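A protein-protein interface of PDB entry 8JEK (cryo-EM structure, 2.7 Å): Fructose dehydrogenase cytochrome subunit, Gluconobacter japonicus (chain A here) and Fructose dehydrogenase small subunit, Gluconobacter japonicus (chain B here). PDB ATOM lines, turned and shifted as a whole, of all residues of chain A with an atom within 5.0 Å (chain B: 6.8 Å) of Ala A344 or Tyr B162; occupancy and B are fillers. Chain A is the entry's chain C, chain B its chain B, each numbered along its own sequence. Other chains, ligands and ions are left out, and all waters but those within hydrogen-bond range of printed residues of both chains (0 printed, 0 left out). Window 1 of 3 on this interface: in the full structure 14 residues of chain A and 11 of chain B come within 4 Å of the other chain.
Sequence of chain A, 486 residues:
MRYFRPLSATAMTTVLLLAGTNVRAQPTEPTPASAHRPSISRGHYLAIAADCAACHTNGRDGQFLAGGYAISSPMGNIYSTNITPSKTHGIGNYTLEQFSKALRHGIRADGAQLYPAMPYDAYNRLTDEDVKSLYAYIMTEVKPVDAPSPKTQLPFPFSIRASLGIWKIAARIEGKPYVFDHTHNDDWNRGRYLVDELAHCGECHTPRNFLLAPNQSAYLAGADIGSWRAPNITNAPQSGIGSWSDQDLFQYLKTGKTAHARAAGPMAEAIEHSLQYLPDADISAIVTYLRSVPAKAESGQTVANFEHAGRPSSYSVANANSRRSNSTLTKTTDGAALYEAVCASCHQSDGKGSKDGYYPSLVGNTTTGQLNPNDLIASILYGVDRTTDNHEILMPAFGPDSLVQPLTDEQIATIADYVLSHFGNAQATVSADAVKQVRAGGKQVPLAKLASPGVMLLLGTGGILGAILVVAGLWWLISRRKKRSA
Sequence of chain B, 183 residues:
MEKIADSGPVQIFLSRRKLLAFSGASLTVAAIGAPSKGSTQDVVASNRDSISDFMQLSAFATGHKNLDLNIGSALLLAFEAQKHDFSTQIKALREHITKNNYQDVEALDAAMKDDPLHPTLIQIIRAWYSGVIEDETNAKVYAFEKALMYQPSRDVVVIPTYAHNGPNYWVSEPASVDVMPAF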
ATOM      1  N   TYR A 315      14.762  34.084  -2.053  1.00  0.00           N
ATOM      2  CA  TYR A 315      15.389  35.392  -1.979  1.00  0.00           C
ATOM      3  C   TYR A 315      14.715  36.351  -2.959  1.00  0.00           C
ATOM      4  O   TYR A 315      13.730  36.012  -3.622  1.00  0.00           O
ATOM      5  CB  TYR A 315      16.895  35.257  -2.233  1.00  0.00           C
ATOM      6  CG  TYR A 315      17.334  35.349  -3.676  1.00  0.00           C
ATOM      7  CD1 TYR A 315      16.719  34.599  -4.670  1.00  0.00           C
ATOM      8  CD2 TYR A 315      18.387  36.176  -4.040  1.00  0.00           C
ATOM      9  CE1 TYR A 315      17.125  34.691  -5.986  1.00  0.00           C
ATOM     10  CE2 TYR A 315      18.802  36.271  -5.347  1.00  0.00           C
ATOM     11  CZ  TYR A 315      18.169  35.527  -6.317  1.00  0.00           C
ATOM     12  OH  TYR A 315      18.585  35.619  -7.624  1.00  0.00           O
ATOM     13  N   TYR A 339      22.657  32.119   0.662  1.00  0.00           N
ATOM     14  CA  TYR A 339      22.381  30.791   0.125  1.00  0.00           C
ATOM     15  C   TYR A 339      22.361  30.812  -1.395  1.00  0.00           C
ATOM     16  O   TYR A 339      22.887  29.901  -2.043  1.00  0.00           O
ATOM     17  CB  TYR A 339      21.054  30.256   0.666  1.00  0.00           C
ATOM     18  CG  TYR A 339      20.588  28.990  -0.028  1.00  0.00           C
ATOM     19  CD1 TYR A 339      21.019  27.742   0.398  1.00  0.00           C
ATOM     20  CD2 TYR A 339      19.720  29.045  -1.109  1.00  0.00           C
ATOM     21  CE1 TYR A 339      20.604  26.589  -0.238  1.00  0.00           C
ATOM     22  CE2 TYR A 339      19.303  27.900  -1.749  1.00  0.00           C
ATOM     23  CZ  TYR A 339      19.744  26.676  -1.310  1.00  0.00           C
ATOM     24  OH  TYR A 339      19.322  25.536  -1.949  1.00  0.00           O
ATOM     25  N   GLU A 340      21.748  31.839  -1.985  1.00  0.00           N
ATOM     26  CA  GLU A 340      21.677  31.914  -3.439  1.00  0.00           C
ATOM     27  C   GLU A 340      23.060  32.066  -4.056  1.00  0.00           C
ATOM     28  O   GLU A 340      23.357  31.458  -5.091  1.00  0.00           O
ATOM     29  CB  GLU A 340      20.770  33.063  -3.863  1.00  0.00           C
ATOM     30  CG  GLU A 340      20.366  33.011  -5.320  1.00  0.00           C
ATOM     31  CD  GLU A 340      19.263  32.013  -5.581  1.00  0.00           C
ATOM     32  OE1 GLU A 340      18.636  31.549  -4.607  1.00  0.00           O
ATOM     33  OE2 GLU A 340      19.019  31.693  -6.760  1.00  0.00           O
ATOM     34  N   VAL A 342      26.099  31.269  -2.681  1.00  0.00           N
ATOM     35  CA  VAL A 342      27.087  30.246  -2.356  1.00  0.00           C
ATOM     36  C   VAL A 342      26.561  28.846  -2.647  1.00  0.00           C
ATOM     37  O   VAL A 342      27.310  27.979  -3.111  1.00  0.00           O
ATOM     38  CB  VAL A 342      27.536  30.365  -0.888  1.00  0.00           C
ATOM     39  CG1 VAL A 342      28.713  29.452  -0.619  1.00  0.00           C
ATOM     40  CG2 VAL A 342      27.902  31.800  -0.563  1.00  0.00           C
ATOM     41  N   CYS A 343      25.278  28.609  -2.391  1.00  0.00           N
ATOM     42  CA  CYS A 343      24.748  27.252  -2.370  1.00  0.00           C
ATOM     43  C   CYS A 343      23.753  26.937  -3.477  1.00  0.00           C
ATOM     44  O   CYS A 343      23.588  25.763  -3.807  1.00  0.00           O
ATOM     45  CB  CYS A 343      24.074  26.968  -1.019  1.00  0.00           C
ATOM     46  SG  CYS A 343      24.920  27.663   0.417  1.00  0.00           S
ATOM     47  N   ALA A 344      23.092  27.936  -4.061  1.00  0.00           N
ATOM     48  CA  ALA A 344      21.965  27.672  -4.949  1.00  0.00           C
ATOM     49  C   ALA A 344      22.367  27.144  -6.321  1.00  0.00           C
ATOM     50  O   ALA A 344      21.483  26.754  -7.091  1.00  0.00           O
ATOM     51  CB  ALA A 344      21.118  28.929  -5.129  1.00  0.00           C
ATOM     52  N   SER A 345      23.656  27.128  -6.657  1.00  0.00           N
ATOM     53  CA  SER A 345      24.057  26.611  -7.961  1.00  0.00           C
ATOM     54  C   SER A 345      23.789  25.116  -8.072  1.00  0.00           C
ATOM     55  O   SER A 345      23.301  24.643  -9.104  1.00  0.00           O
ATOM     56  CB  SER A 345      25.532  26.911  -8.214  1.00  0.00           C
ATOM     57  OG  SER A 345      25.989  26.246  -9.376  1.00  0.00           O
ATOM     58  N   CYS A 346      24.103  24.357  -7.023  1.00  0.00           N
ATOM     59  CA  CYS A 346      23.967  22.904  -7.044  1.00  0.00           C
ATOM     60  C   CYS A 346      22.644  22.447  -6.438  1.00  0.00           C
ATOM     61  O   CYS A 346      21.836  21.802  -7.112  1.00  0.00           O
ATOM     62  CB  CYS A 346      25.154  22.277  -6.315  1.00  0.00           C
ATOM     63  SG  CYS A 346      26.711  22.713  -7.083  1.00  0.00           S
ATOM     64  N   HIS A 347      22.415  22.759  -5.166  1.00  0.00           N
ATOM     65  CA  HIS A 347      21.069  22.668  -4.625  1.00  0.00           C
ATOM     66  C   HIS A 347      20.257  23.824  -5.177  1.00  0.00           C
ATOM     67  O   HIS A 347      20.691  24.973  -5.133  1.00  0.00           O
ATOM     68  CB  HIS A 347      21.088  22.720  -3.099  1.00  0.00           C
ATOM     69  CG  HIS A 347      22.180  21.908  -2.478  1.00  0.00           C
ATOM     70  ND1 HIS A 347      22.103  20.541  -2.333  1.00  0.00           N
ATOM     71  CD2 HIS A 347      23.374  22.275  -1.958  1.00  0.00           C
ATOM     72  CE1 HIS A 347      23.204  20.100  -1.754  1.00  0.00           C
ATOM     73  NE2 HIS A 347      23.991  21.132  -1.516  1.00  0.00           N
ATOM     74  N   GLN A 348      19.078  23.528  -5.705  1.00  0.00           N
ATOM     75  CA  GLN A 348      18.358  24.547  -6.451  1.00  0.00           C
ATOM     76  C   GLN A 348      17.913  25.673  -5.516  1.00  0.00           C
ATOM     77  O   GLN A 348      18.056  25.601  -4.292  1.00  0.00           O
ATOM     78  CB  GLN A 348      17.185  23.916  -7.192  1.00  0.00           C
ATOM     79  CG  GLN A 348      17.614  22.982  -8.315  1.00  0.00           C
ATOM     80  CD  GLN A 348      18.901  23.424  -8.997  1.00  0.00           C
ATOM     81  OE1 GLN A 348      18.985  24.524  -9.543  1.00  0.00           O
ATOM     82  NE2 GLN A 348      19.907  22.561  -8.975  1.00  0.00           N
ATOM     83  N   SER A 349      17.387  26.747  -6.112  1.00  0.00           N
ATOM     84  CA  SER A 349      16.972  27.902  -5.323  1.00  0.00           C
ATOM     85  C   SER A 349      15.888  27.539  -4.319  1.00  0.00           C
ATOM     86  O   SER A 349      15.835  28.118  -3.228  1.00  0.00           O
ATOM     87  CB  SER A 349      16.491  29.022  -6.242  1.00  0.00           C
ATOM     88  OG  SER A 349      16.418  30.253  -5.547  1.00  0.00           O
ATOM     89  N   PHE B 144      16.083  36.804 -12.842  1.00  0.00           N
ATOM     90  CA  PHE B 144      17.000  35.921 -13.544  1.00  0.00           C
ATOM     91  C   PHE B 144      16.739  34.499 -13.080  1.00  0.00           C
ATOM     92  O   PHE B 144      16.535  34.257 -11.886  1.00  0.00           O
ATOM     93  CB  PHE B 144      18.461  36.297 -13.294  1.00  0.00           C
ATOM     94  CG  PHE B 144      19.441  35.325 -13.886  1.00  0.00           C
ATOM     95  CD1 PHE B 144      19.534  35.164 -15.257  1.00  0.00           C
ATOM     96  CD2 PHE B 144      20.257  34.564 -13.073  1.00  0.00           C
ATOM     97  CE1 PHE B 144      20.430  34.268 -15.802  1.00  0.00           C
ATOM     98  CE2 PHE B 144      21.151  33.669 -13.615  1.00  0.00           C
ATOM     99  CZ  PHE B 144      21.237  33.523 -14.982  1.00  0.00           C
ATOM    100  N   GLU B 145      16.725  33.566 -14.031  1.00  0.00           N
ATOM    101  CA  GLU B 145      16.422  32.149 -13.879  1.00  0.00           C
ATOM    102  C   GLU B 145      14.925  31.938 -13.654  1.00  0.00           C
ATOM    103  O   GLU B 145      14.456  30.806 -13.752  1.00  0.00           O
ATOM    104  CB  GLU B 145      17.218  31.474 -12.743  1.00  0.00           C
ATOM    105  CG  GLU B 145      17.203  29.957 -12.750  1.00  0.00           C
ATOM    106  CD  GLU B 145      16.855  29.372 -11.400  1.00  0.00           C
ATOM    107  OE1 GLU B 145      16.761  30.143 -10.424  1.00  0.00           O
ATOM    108  OE2 GLU B 145      16.684  28.139 -11.314  1.00  0.00           O
ATOM    109  N   ARG B 154      14.300  25.672 -21.362  1.00  0.00           N
ATOM    110  CA  ARG B 154      14.864  25.309 -20.066  1.00  0.00           C
ATOM    111  C   ARG B 154      15.071  23.809 -19.916  1.00  0.00           C
ATOM    112  O   ARG B 154      15.963  23.390 -19.172  1.00  0.00           O
ATOM    113  CB  ARG B 154      13.961  25.819 -18.943  1.00  0.00           C
ATOM    114  CG  ARG B 154      14.595  25.764 -17.570  1.00  0.00           C
ATOM    115  CD  ARG B 154      13.781  26.533 -16.553  1.00  0.00           C
ATOM    116  NE  ARG B 154      14.400  26.504 -15.234  1.00  0.00           N
ATOM    117  CZ  ARG B 154      14.004  27.242 -14.208  1.00  0.00           C
ATOM    118  NH1 ARG B 154      12.990  28.084 -14.312  1.00  0.00           N
ATOM    119  NH2 ARG B 154      14.643  27.136 -13.047  1.00  0.00           N
ATOM    120  N   VAL B 158      21.023  25.079 -20.316  1.00  0.00           N
ATOM    121  CA  VAL B 158      21.292  25.490 -18.946  1.00  0.00           C
ATOM    122  C   VAL B 158      21.064  26.989 -18.796  1.00  0.00           C
ATOM    123  O   VAL B 158      21.318  27.773 -19.720  1.00  0.00           O
ATOM    124  CB  VAL B 158      22.728  25.096 -18.558  1.00  0.00           C
ATOM    125  CG1 VAL B 158      23.744  25.856 -19.395  1.00  0.00           C
ATOM    126  CG2 VAL B 158      22.978  25.331 -17.089  1.00  0.00           C
ATOM    127  N   ILE B 159      20.548  27.391 -17.639  1.00  0.00           N
ATOM    128  CA  ILE B 159      20.609  28.787 -17.222  1.00  0.00           C
ATOM    129  C   ILE B 159      21.926  28.920 -16.468  1.00  0.00           C
ATOM    130  O   ILE B 159      22.043  28.426 -15.338  1.00  0.00           O
ATOM    131  CB  ILE B 159      19.392  29.184 -16.371  1.00  0.00           C
ATOM    132  CG1 ILE B 159      18.101  28.888 -17.135  1.00  0.00           C
ATOM    133  CG2 ILE B 159      19.453  30.651 -16.003  1.00  0.00           C
ATOM    134  CD1 ILE B 159      16.855  29.052 -16.313  1.00  0.00           C
ATOM    135  N   PRO B 160      22.930  29.588 -17.053  1.00  0.00           N
ATOM    136  CA  PRO B 160      24.335  29.306 -16.718  1.00  0.00           C
ATOM    137  C   PRO B 160      24.705  29.142 -15.249  1.00  0.00           C
ATOM    138  O   PRO B 160      25.174  28.069 -14.863  1.00  0.00           O
ATOM    139  CB  PRO B 160      25.054  30.507 -17.333  1.00  0.00           C
ATOM    140  CG  PRO B 160      24.279  30.743 -18.580  1.00  0.00           C
ATOM    141  CD  PRO B 160      22.830  30.496 -18.209  1.00  0.00           C
ATOM    142  N   THR B 161      24.482  30.138 -14.413  1.00  0.00           N
ATOM    143  CA  THR B 161      25.051  29.947 -13.073  1.00  0.00           C
ATOM    144  C   THR B 161      24.293  28.929 -12.217  1.00  0.00           C
ATOM    145  O   THR B 161      24.653  28.753 -11.049  1.00  0.00           O
ATOM    146  CB  THR B 161      25.127  31.283 -12.341  1.00  0.00           C
ATOM    147  OG1 THR B 161      23.999  32.088 -12.701  1.00  0.00           O
ATOM    148  CG2 THR B 161      26.418  32.007 -12.687  1.00  0.00           C
ATOM    149  N   TYR B 162      23.276  28.263 -12.754  1.00  0.00           N
ATOM    150  CA  TYR B 162      22.555  27.209 -12.060  1.00  0.00           C
ATOM    151  C   TYR B 162      22.708  25.917 -12.847  1.00  0.00           C
ATOM    152  O   TYR B 162      22.798  25.931 -14.075  1.00  0.00           O
ATOM    153  CB  TYR B 162      21.077  27.565 -11.890  1.00  0.00           C
ATOM    154  CG  TYR B 162      20.858  28.832 -11.100  1.00  0.00           C
ATOM    155  CD1 TYR B 162      20.839  30.070 -11.726  1.00  0.00           C
ATOM    156  CD2 TYR B 162      20.690  28.792  -9.723  1.00  0.00           C
ATOM    157  CE1 TYR B 162      20.646  31.228 -11.007  1.00  0.00           C
ATOM    158  CE2 TYR B 162      20.498  29.945  -8.997  1.00  0.00           C
ATOM    159  CZ  TYR B 162      20.476  31.161  -9.642  1.00  0.00           C
ATOM    160  OH  TYR B 162      20.285  32.314  -8.918  1.00  0.00           O
ATOM    161  N   ALA B 163      22.734  24.798 -12.134  1.00  0.00           N
ATOM    162  CA  ALA B 163      23.140  23.522 -12.707  1.00  0.00           C
ATOM    163  C   ALA B 163      21.939  22.720 -13.186  1.00  0.00           C
ATOM    164  O   ALA B 163      20.929  22.617 -12.481  1.00  0.00           O
ATOM    165  CB  ALA B 163      23.934  22.705 -11.687  1.00  0.00           C
ATOM    166  N   HIS B 164      22.051  22.166 -14.390  1.00  0.00           N
ATOM    167  CA  HIS B 164      21.225  21.042 -14.797  1.00  0.00           C
ATOM    168  C   HIS B 164      21.609  19.803 -13.985  1.00  0.00           C
ATOM    169  O   HIS B 164      22.581  19.799 -13.223  1.00  0.00           O
ATOM    170  CB  HIS B 164      21.394  20.774 -16.291  1.00  0.00           C
ATOM    171  CG  HIS B 164      20.184  21.084 -17.116  1.00  0.00           C
ATOM    172  ND1 HIS B 164      19.351  20.104 -17.610  1.00  0.00           N
ATOM    173  CD2 HIS B 164      19.676  22.261 -17.548  1.00  0.00           C
ATOM    174  CE1 HIS B 164      18.379  20.664 -18.307  1.00  0.00           C
ATOM    175  NE2 HIS B 164      18.552  21.972 -18.283  1.00  0.00           N
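The backbone carbonyl oxygen (O) of Thr B161 is in hydrogen-bond range of the side-chain hydroxyl (OG) of Ser A345 (3.3 Å).
The side-chain hydroxyl (OH) of Tyr B162 is in hydrogen-bond range of the side-chain carboxylate (OE2) of Glu A340 (2.6 Å).
The backbone carbonyl oxygen of Ser A345 is in hydrogen-bond range of the backbone NH of Ala B163.
The backbone NH of Ala A344 sits at hydrogen-bond distance from the backbone carbonyl oxygen of Tyr A339 (2.8 Å).
The side-chain hydroxyl of Tyr A339 sits at hydrogen-bond distance from the backbone carbonyl oxygen of Gln A348 (2.7 Å).
The side-chain carboxylate of Glu A340 sits at hydrogen-bond distance from the side-chain hydroxyl of Ser A349 (2.7 Å).
O of Cys A346 lies within hydrogen-bond range of NE2 of Gln A348.
Tyr A315 touches Tyr B162 (OH to OH, 3.9 Å).
O of Ala A344 touches CD2 of Tyr B162 (3.4 Å).
Tyr B162 touches Ser A345.
Gln A348 touches Ala B163 (NE2 to O, 3.7 Å).
Of the printed residues of chain B, Ala A344 touches Tyr B162 (3.4 Å).
Printed residues of chain A within 4 Å of Tyr B162: Tyr A315, Glu A340, Ala A344 and Ser A345.
Of the printed residues of chain B, Ser A345 touches Thr B161, Tyr B162 and Ala B163.
Printed residues of chain B within 4 Å of Tyr A315: Tyr B162 (3.9 Å).
Of the printed residues of chain B, Gln A348 touches Ala B163 (3.7 Å).
Of the printed residues of chain A, Thr B161 touches Ser A345.
Of the printed residues of chain B, Glu A340 touches Tyr B162 (2.6 Å).
The nearest residue of chain B that does not touch Ala A344 is Thr B161 (5.5 Å).
The nearest printed residue of chain B that does not touch Ser A345 is Pro B160 (5.8 Å).
Of the 11 printed residues of chain A, 5 touch a printed residue of chain B.
Printed residues of chain A that touch a printed residue of chain B: Tyr A315, Glu A340, Ala A344, Ser A345 and Gln A348.
Of the 10 printed residues of chain B, 3 touch a printed residue of chain A.
Among the printed residues, 7 pairs touch across the chains.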
